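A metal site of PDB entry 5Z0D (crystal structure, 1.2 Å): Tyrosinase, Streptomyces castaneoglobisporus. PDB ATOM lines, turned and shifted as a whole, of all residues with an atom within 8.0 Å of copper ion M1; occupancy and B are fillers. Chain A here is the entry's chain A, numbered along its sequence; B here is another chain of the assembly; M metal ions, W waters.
ND1 of His 63 sits close to O of Gly 53, 3.3 Å away.
The backbone carbonyl oxygen (O) of Gly 204 is in hydrogen-bond range of a ring nitrogen (ND1) of His 38 (3.0 Å).
A ring nitrogen (ND1) of His 63 is in hydrogen-bond range of the backbone carbonyl oxygen of Phe 59, at 2.8 Å.
ND1 of His 54 lies within hydrogen-bond range of OD1 of Asp 45 (2.8 Å).
Copper ion M1 is bound by a ring nitrogen (NE2) of His 63 (1.9 Å), a ring nitrogen (NE2) of His 38 (1.9 Å), a ring nitrogen (NE2) of His 54 (2.1 Å) and water W1 (2.6 Å).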
ATOM      1  N   THR A  37     -21.376  12.358  18.003  1.00  0.00           N
ATOM      2  CA  THR A  37     -20.771  13.708  17.954  1.00  0.00           C
ATOM      3  C   THR A  37     -19.402  13.672  18.626  1.00  0.00           C
ATOM      4  O   THR A  37     -18.412  14.245  18.134  1.00  0.00           O
ATOM      5  CB  THR A  37     -21.738  14.681  18.628  1.00  0.00           C
ATOM      6  OG1 THR A  37     -22.940  14.772  17.844  1.00  0.00           O
ATOM      7  CG2 THR A  37     -21.096  16.087  18.735  1.00  0.00           C
ATOM      8  N   HIS A  38     -19.333  13.011  19.779  1.00  0.00           N
ATOM      9  CA  HIS A  38     -18.077  12.964  20.509  1.00  0.00           C
ATOM     10  C   HIS A  38     -16.974  12.325  19.676  1.00  0.00           C
ATOM     11  O   HIS A  38     -15.846  12.881  19.589  1.00  0.00           O
ATOM     12  CB  HIS A  38     -18.259  12.189  21.828  1.00  0.00           C
ATOM     13  CG  HIS A  38     -17.021  12.352  22.666  1.00  0.00           C
ATOM     14  ND1 HIS A  38     -16.005  11.444  22.747  1.00  0.00           N
ATOM     15  CD2 HIS A  38     -16.671  13.400  23.439  1.00  0.00           C
ATOM     16  CE1 HIS A  38     -15.056  11.936  23.563  1.00  0.00           C
ATOM     17  NE2 HIS A  38     -15.429  13.154  24.019  1.00  0.00           N
ATOM     18  N   ASN A  39     -17.233  11.188  19.081  1.00  0.00           N
ATOM     19  CA  ASN A  39     -16.178  10.502  18.294  1.00  0.00           C
ATOM     20  C   ASN A  39     -15.790  11.319  17.098  1.00  0.00           C
ATOM     21  O   ASN A  39     -14.601  11.310  16.720  1.00  0.00           O
ATOM     22  CB  ASN A  39     -16.653   9.107  17.899  1.00  0.00           C
ATOM     23  CG  ASN A  39     -15.506   8.204  17.466  1.00  0.00           C
ATOM     24  OD1 ASN A  39     -14.440   8.203  18.094  1.00  0.00           O
ATOM     25  ND2 ASN A  39     -15.746   7.411  16.424  1.00  0.00           N
ATOM     26  N   PHE A  41     -15.561  14.591  16.925  1.00  0.00           N
ATOM     27  CA  PHE A  41     -14.566  15.556  17.389  1.00  0.00           C
ATOM     28  C   PHE A  41     -13.298  14.875  17.811  1.00  0.00           C
ATOM     29  O   PHE A  41     -12.187  15.373  17.521  1.00  0.00           O
ATOM     30  CB  PHE A  41     -15.140  16.444  18.541  1.00  0.00           C
ATOM     31  CG  PHE A  41     -15.947  17.576  17.938  1.00  0.00           C
ATOM     32  CD1 PHE A  41     -15.372  18.827  17.667  1.00  0.00           C
ATOM     33  CD2 PHE A  41     -17.290  17.351  17.597  1.00  0.00           C
ATOM     34  CE1 PHE A  41     -16.110  19.870  17.055  1.00  0.00           C
ATOM     35  CE2 PHE A  41     -18.034  18.341  16.962  1.00  0.00           C
ATOM     36  CZ  PHE A  41     -17.437  19.572  16.685  1.00  0.00           C
ATOM     37  N   ILE A  42     -13.341  13.675  18.446  1.00  0.00           N
ATOM     38  CA  ILE A  42     -12.105  12.975  18.774  1.00  0.00           C
ATOM     39  C   ILE A  42     -11.287  12.723  17.553  1.00  0.00           C
ATOM     40  O   ILE A  42     -10.034  12.879  17.550  1.00  0.00           O
ATOM     41  CB  ILE A  42     -12.428  11.638  19.530  1.00  0.00           C
ATOM     42  CG1 ILE A  42     -12.897  11.888  20.949  1.00  0.00           C
ATOM     43  CG2 ILE A  42     -11.263  10.616  19.466  1.00  0.00           C
ATOM     44  CD1 ILE A  42     -11.787  12.300  21.907  1.00  0.00           C
ATOM     45  N   ASP A  45     -10.165  16.667  15.981  1.00  0.00           N
ATOM     46  CA  ASP A  45      -9.321  17.605  16.710  1.00  0.00           C
ATOM     47  C   ASP A  45      -7.862  17.165  16.608  1.00  0.00           C
ATOM     48  O   ASP A  45      -7.513  16.094  17.136  1.00  0.00           O
ATOM     49  CB  ASP A  45      -9.722  17.684  18.190  1.00  0.00           C
ATOM     50  CG  ASP A  45     -11.105  18.297  18.425  1.00  0.00           C
ATOM     51  OD1 ASP A  45     -11.758  17.874  19.441  1.00  0.00           O
ATOM     52  OD2 ASP A  45     -11.548  19.192  17.650  1.00  0.00           O
ATOM     53  N   GLY A  53     -12.782  20.408  20.436  1.00  0.00           N
ATOM     54  CA  GLY A  53     -13.291  19.743  21.631  1.00  0.00           C
ATOM     55  C   GLY A  53     -12.193  19.251  22.552  1.00  0.00           C
ATOM     56  O   GLY A  53     -12.459  19.026  23.732  1.00  0.00           O
ATOM     57  N   HIS A  54     -10.993  19.004  22.024  1.00  0.00           N
ATOM     58  CA  HIS A  54      -9.942  18.292  22.759  1.00  0.00           C
ATOM     59  C   HIS A  54      -8.592  18.940  22.403  1.00  0.00           C
ATOM     60  O   HIS A  54      -8.495  19.681  21.411  1.00  0.00           O
ATOM     61  CB  HIS A  54      -9.875  16.775  22.349  1.00  0.00           C
ATOM     62  CG  HIS A  54     -11.229  16.124  22.610  1.00  0.00           C
ATOM     63  ND1 HIS A  54     -12.244  16.138  21.644  1.00  0.00           N
ATOM     64  CD2 HIS A  54     -11.768  15.560  23.714  1.00  0.00           C
ATOM     65  CE1 HIS A  54     -13.318  15.563  22.173  1.00  0.00           C
ATOM     66  NE2 HIS A  54     -13.065  15.184  23.440  1.00  0.00           N
ATOM     67  N   PHE A  59     -11.104  22.625  25.121  1.00  0.00           N
ATOM     68  CA  PHE A  59     -11.472  21.366  25.761  1.00  0.00           C
ATOM     69  C   PHE A  59     -12.442  21.592  26.931  1.00  0.00           C
ATOM     70  O   PHE A  59     -13.452  20.887  27.052  1.00  0.00           O
ATOM     71  CB  PHE A  59     -10.176  20.708  26.285  1.00  0.00           C
ATOM     72  CG  PHE A  59     -10.362  19.507  27.194  1.00  0.00           C
ATOM     73  CD1 PHE A  59     -10.881  18.303  26.723  1.00  0.00           C
ATOM     74  CD2 PHE A  59      -9.984  19.593  28.539  1.00  0.00           C
ATOM     75  CE1 PHE A  59     -10.977  17.192  27.538  1.00  0.00           C
ATOM     76  CE2 PHE A  59     -10.100  18.478  29.379  1.00  0.00           C
ATOM     77  CZ  PHE A  59     -10.620  17.291  28.869  1.00  0.00           C
ATOM     78  N   TRP A  62     -15.885  23.397  25.842  1.00  0.00           N
ATOM     79  CA  TRP A  62     -16.609  22.494  24.945  1.00  0.00           C
ATOM     80  C   TRP A  62     -17.271  21.391  25.712  1.00  0.00           C
ATOM     81  O   TRP A  62     -18.456  21.080  25.526  1.00  0.00           O
ATOM     82  CB  TRP A  62     -15.628  21.932  23.886  1.00  0.00           C
ATOM     83  CG  TRP A  62     -16.332  21.203  22.777  1.00  0.00           C
ATOM     84  CD1 TRP A  62     -16.692  21.778  21.598  1.00  0.00           C
ATOM     85  CD2 TRP A  62     -16.758  19.819  22.709  1.00  0.00           C
ATOM     86  NE1 TRP A  62     -17.319  20.832  20.800  1.00  0.00           N
ATOM     87  CE2 TRP A  62     -17.367  19.618  21.459  1.00  0.00           C
ATOM     88  CE3 TRP A  62     -16.664  18.704  23.592  1.00  0.00           C
ATOM     89  CZ2 TRP A  62     -17.904  18.380  21.081  1.00  0.00           C
ATOM     90  CZ3 TRP A  62     -17.192  17.493  23.223  1.00  0.00           C
ATOM     91  CH2 TRP A  62     -17.814  17.316  21.959  1.00  0.00           C
ATOM     92  N   HIS A  63     -16.498  20.726  26.624  1.00  0.00           N
ATOM     93  CA  HIS A  63     -17.154  19.676  27.414  1.00  0.00           C
ATOM     94  C   HIS A  63     -18.163  20.240  28.377  1.00  0.00           C
ATOM     95  O   HIS A  63     -19.142  19.560  28.694  1.00  0.00           O
ATOM     96  CB  HIS A  63     -16.083  18.814  28.142  1.00  0.00           C
ATOM     97  CG  HIS A  63     -15.398  17.880  27.191  1.00  0.00           C
ATOM     98  ND1 HIS A  63     -14.336  18.275  26.389  1.00  0.00           N
ATOM     99  CD2 HIS A  63     -15.627  16.579  26.867  1.00  0.00           C
ATOM    100  CE1 HIS A  63     -13.948  17.245  25.644  1.00  0.00           C
ATOM    101  NE2 HIS A  63     -14.710  16.150  25.877  1.00  0.00           N
ATOM    102  N   PHE A  66     -21.175  20.456  26.159  1.00  0.00           N
ATOM    103  CA  PHE A  66     -21.636  19.117  25.792  1.00  0.00           C
ATOM    104  C   PHE A  66     -22.354  18.499  26.955  1.00  0.00           C
ATOM    105  O   PHE A  66     -23.459  17.913  26.806  1.00  0.00           O
ATOM    106  CB  PHE A  66     -20.372  18.317  25.404  1.00  0.00           C
ATOM    107  CG  PHE A  66     -20.642  16.967  24.768  1.00  0.00           C
ATOM    108  CD1 PHE A  66     -21.334  16.843  23.592  1.00  0.00           C
ATOM    109  CD2 PHE A  66     -20.122  15.805  25.343  1.00  0.00           C
ATOM    110  CE1 PHE A  66     -21.483  15.594  22.993  1.00  0.00           C
ATOM    111  CE2 PHE A  66     -20.299  14.587  24.755  1.00  0.00           C
ATOM    112  CZ  PHE A  66     -20.966  14.458  23.583  1.00  0.00           C
ATOM    113  N   LEU A  67     -21.826  18.609  28.175  1.00  0.00           N
ATOM    114  CA  LEU A  67     -22.513  18.102  29.360  1.00  0.00           C
ATOM    115  C   LEU A  67     -23.813  18.828  29.655  1.00  0.00           C
ATOM    116  O   LEU A  67     -24.778  18.195  30.061  1.00  0.00           O
ATOM    117  CB  LEU A  67     -21.584  18.179  30.582  1.00  0.00           C
ATOM    118  CG  LEU A  67     -20.831  16.827  30.855  1.00  0.00           C
ATOM    119  CD1 LEU A  67     -19.962  16.415  29.671  1.00  0.00           C
ATOM    120  CD2 LEU A  67     -20.028  17.014  32.143  1.00  0.00           C
ATOM    121  N   GLU A 182      -6.182  17.992  31.211  1.00  0.00           N
ATOM    122  CA  GLU A 182      -6.545  17.033  30.161  1.00  0.00           C
ATOM    123  C   GLU A 182      -5.681  15.812  30.235  1.00  0.00           C
ATOM    124  O   GLU A 182      -6.168  14.667  30.139  1.00  0.00           O
ATOM    125  CB  GLU A 182      -6.464  17.801  28.814  1.00  0.00           C
ATOM    126  CG  GLU A 182      -7.069  16.885  27.681  1.00  0.00           C
ATOM    127  CD  GLU A 182      -7.142  17.635  26.362  1.00  0.00           C
ATOM    128  OE1 GLU A 182      -6.788  18.845  26.264  1.00  0.00           O
ATOM    129  OE2 GLU A 182      -7.553  16.921  25.382  1.00  0.00           O
ATOM    130  N   HIS A 190      -7.111  13.707  33.423  1.00  0.00           N
ATOM    131  CA  HIS A 190      -8.318  13.236  32.733  1.00  0.00           C
ATOM    132  C   HIS A 190      -8.081  12.061  31.795  1.00  0.00           C
ATOM    133  O   HIS A 190      -8.892  11.132  31.769  1.00  0.00           O
ATOM    134  CB  HIS A 190      -8.949  14.442  31.982  1.00  0.00           C
ATOM    135  CG  HIS A 190      -9.697  14.076  30.738  1.00  0.00           C
ATOM    136  ND1 HIS A 190      -9.026  13.891  29.537  1.00  0.00           N
ATOM    137  CD2 HIS A 190     -10.991  13.861  30.514  1.00  0.00           C
ATOM    138  CE1 HIS A 190      -9.956  13.571  28.592  1.00  0.00           C
ATOM    139  NE2 HIS A 190     -11.173  13.524  29.156  1.00  0.00           N
ATOM    140  N   HIS A 194      -9.740   7.843  31.826  1.00  0.00           N
ATOM    141  CA  HIS A 194     -10.254   7.063  30.692  1.00  0.00           C
ATOM    142  C   HIS A 194      -9.548   5.734  30.584  1.00  0.00           C
ATOM    143  O   HIS A 194     -10.177   4.657  30.393  1.00  0.00           O
ATOM    144  CB  HIS A 194     -10.101   7.878  29.406  1.00  0.00           C
ATOM    145  CG  HIS A 194     -11.098   8.920  29.123  1.00  0.00           C
ATOM    146  ND1 HIS A 194     -12.318   8.576  28.519  1.00  0.00           N
ATOM    147  CD2 HIS A 194     -11.116  10.263  29.245  1.00  0.00           C
ATOM    148  CE1 HIS A 194     -12.971   9.705  28.325  1.00  0.00           C
ATOM    149  NE2 HIS A 194     -12.324  10.789  28.758  1.00  0.00           N
ATOM    150  N   THR A 203     -11.751   4.700  24.429  1.00  0.00           N
ATOM    151  CA  THR A 203     -11.879   4.914  23.007  1.00  0.00           C
ATOM    152  C   THR A 203     -12.550   6.260  22.709  1.00  0.00           C
ATOM    153  O   THR A 203     -13.085   6.930  23.604  1.00  0.00           O
ATOM    154  CB  THR A 203     -12.731   3.832  22.336  1.00  0.00           C
ATOM    155  OG1 THR A 203     -14.140   4.074  22.636  1.00  0.00           O
ATOM    156  CG2 THR A 203     -12.372   2.429  22.868  1.00  0.00           C
ATOM    157  N   GLY A 204     -12.573   6.661  21.419  1.00  0.00           N
ATOM    158  CA  GLY A 204     -13.321   7.875  21.035  1.00  0.00           C
ATOM    159  C   GLY A 204     -14.808   7.806  21.239  1.00  0.00           C
ATOM    160  O   GLY A 204     -15.447   8.870  21.328  1.00  0.00           O
ATOM    161  N   SER A 206     -16.129   6.874  23.976  1.00  0.00           N
ATOM    162  CA  SER A 206     -16.199   6.797  25.453  1.00  0.00           C
ATOM    163  C   SER A 206     -17.541   7.204  26.047  1.00  0.00           C
ATOM    164  O   SER A 206     -17.878   6.632  27.087  1.00  0.00           O
ATOM    165  CB  SER A 206     -15.033   7.595  26.054  1.00  0.00           C
ATOM    166  OG  SER A 206     -14.956   8.911  25.535  1.00  0.00           O
ATOM    167  N   PRO A 207     -18.365   8.084  25.446  1.00  0.00           N
ATOM    168  CA  PRO A 207     -19.681   8.337  26.050  1.00  0.00           C
ATOM    169  C   PRO A 207     -20.591   7.132  26.001  1.00  0.00           C
ATOM    170  O   PRO A 207     -21.671   7.202  26.606  1.00  0.00           O
ATOM    171  CB  PRO A 207     -20.263   9.517  25.262  1.00  0.00           C
ATOM    172  CG  PRO A 207     -18.998  10.244  24.699  1.00  0.00           C
ATOM    173  CD  PRO A 207     -18.088   9.082  24.385  1.00  0.00           C
ATOM    174  N   PHE A 212     -18.808   8.273  31.668  1.00  0.00           N
ATOM    175  CA  PHE A 212     -18.211   9.395  30.955  1.00  0.00           C
ATOM    176  C   PHE A 212     -18.681  10.706  31.533  1.00  0.00           C
ATOM    177  O   PHE A 212     -17.916  11.649  31.705  1.00  0.00           O
ATOM    178  CB  PHE A 212     -18.601   9.239  29.459  1.00  0.00           C
ATOM    179  CG  PHE A 212     -18.239  10.458  28.628  1.00  0.00           C
ATOM    180  CD1 PHE A 212     -19.031  11.553  28.440  1.00  0.00           C
ATOM    181  CD2 PHE A 212     -16.958  10.462  28.005  1.00  0.00           C
ATOM    182  CE1 PHE A 212     -18.619  12.699  27.737  1.00  0.00           C
ATOM    183  CE2 PHE A 212     -16.549  11.562  27.267  1.00  0.00           C
ATOM    184  CZ  PHE A 212     -17.375  12.650  27.109  1.00  0.00           C
ATOM    185  N   HIS A 216     -16.467  13.599  33.331  1.00  0.00           N
ATOM    186  CA  HIS A 216     -16.386  14.984  32.852  1.00  0.00           C
ATOM    187  C   HIS A 216     -17.055  15.967  33.752  1.00  0.00           C
ATOM    188  O   HIS A 216     -16.611  17.130  33.774  1.00  0.00           O
ATOM    189  CB  HIS A 216     -16.914  15.085  31.387  1.00  0.00           C
ATOM    190  CG  HIS A 216     -15.766  14.783  30.473  1.00  0.00           C
ATOM    191  ND1 HIS A 216     -14.866  15.787  30.106  1.00  0.00           N
ATOM    192  CD2 HIS A 216     -15.322  13.657  29.912  1.00  0.00           C
ATOM    193  CE1 HIS A 216     -13.885  15.216  29.341  1.00  0.00           C
ATOM    194  NE2 HIS A 216     -14.149  13.904  29.211  1.00  0.00           N
ATOM    195  N   HIS B  97      -7.398   5.821  22.549  1.00  0.00           N
ATOM    196  CA  HIS B  97      -7.184   7.225  22.172  1.00  0.00           C
ATOM    197  C   HIS B  97      -6.453   7.980  23.276  1.00  0.00           C
ATOM    198  O   HIS B  97      -5.885   9.050  22.958  1.00  0.00           O
ATOM    199  CB  HIS B  97      -8.600   7.805  21.932  1.00  0.00           C
ATOM    200  CG  HIS B  97      -8.443   9.255  21.674  1.00  0.00           C
ATOM    201  ND1 HIS B  97      -8.092   9.726  20.472  1.00  0.00           N
ATOM    202  CD2 HIS B  97      -8.518  10.384  22.409  1.00  0.00           C
ATOM    203  CE1 HIS B  97      -7.959  10.997  20.357  1.00  0.00           C
ATOM    204  NE2 HIS B  97      -8.204  11.411  21.582  1.00  0.00           N
ATOM    205  N   TYR B  98      -6.477   7.509  24.490  1.00  0.00           N
ATOM    206  CA  TYR B  98      -6.029   8.335  25.634  1.00  0.00           C
ATOM    207  C   TYR B  98      -4.699   7.845  26.129  1.00  0.00           C
ATOM    208  O   TYR B  98      -4.283   8.325  27.177  1.00  0.00           O
ATOM    209  CB  TYR B  98      -7.089   8.337  26.770  1.00  0.00           C
ATOM    210  CG  TYR B  98      -8.462   8.825  26.322  1.00  0.00           C
ATOM    211  CD1 TYR B  98      -9.450   7.961  25.892  1.00  0.00           C
ATOM    212  CD2 TYR B  98      -8.762  10.187  26.288  1.00  0.00           C
ATOM    213  CE1 TYR B  98     -10.690   8.421  25.476  1.00  0.00           C
ATOM    214  CE2 TYR B  98     -10.025  10.628  25.889  1.00  0.00           C
ATOM    215  CZ  TYR B  98     -10.998   9.787  25.484  1.00  0.00           C
ATOM    216  OH  TYR B  98     -12.237  10.198  25.081  1.00  0.00           O
HETATM  217 CU    CU M   1     -14.402  14.520  24.903  1.00  0.00          CU
HETATM  218 CU    CU M   2     -12.844  12.652  28.433  1.00  0.00          CU
HETATM  219  O   HOH W   1     -12.632  13.099  26.078  1.00  0.00           O
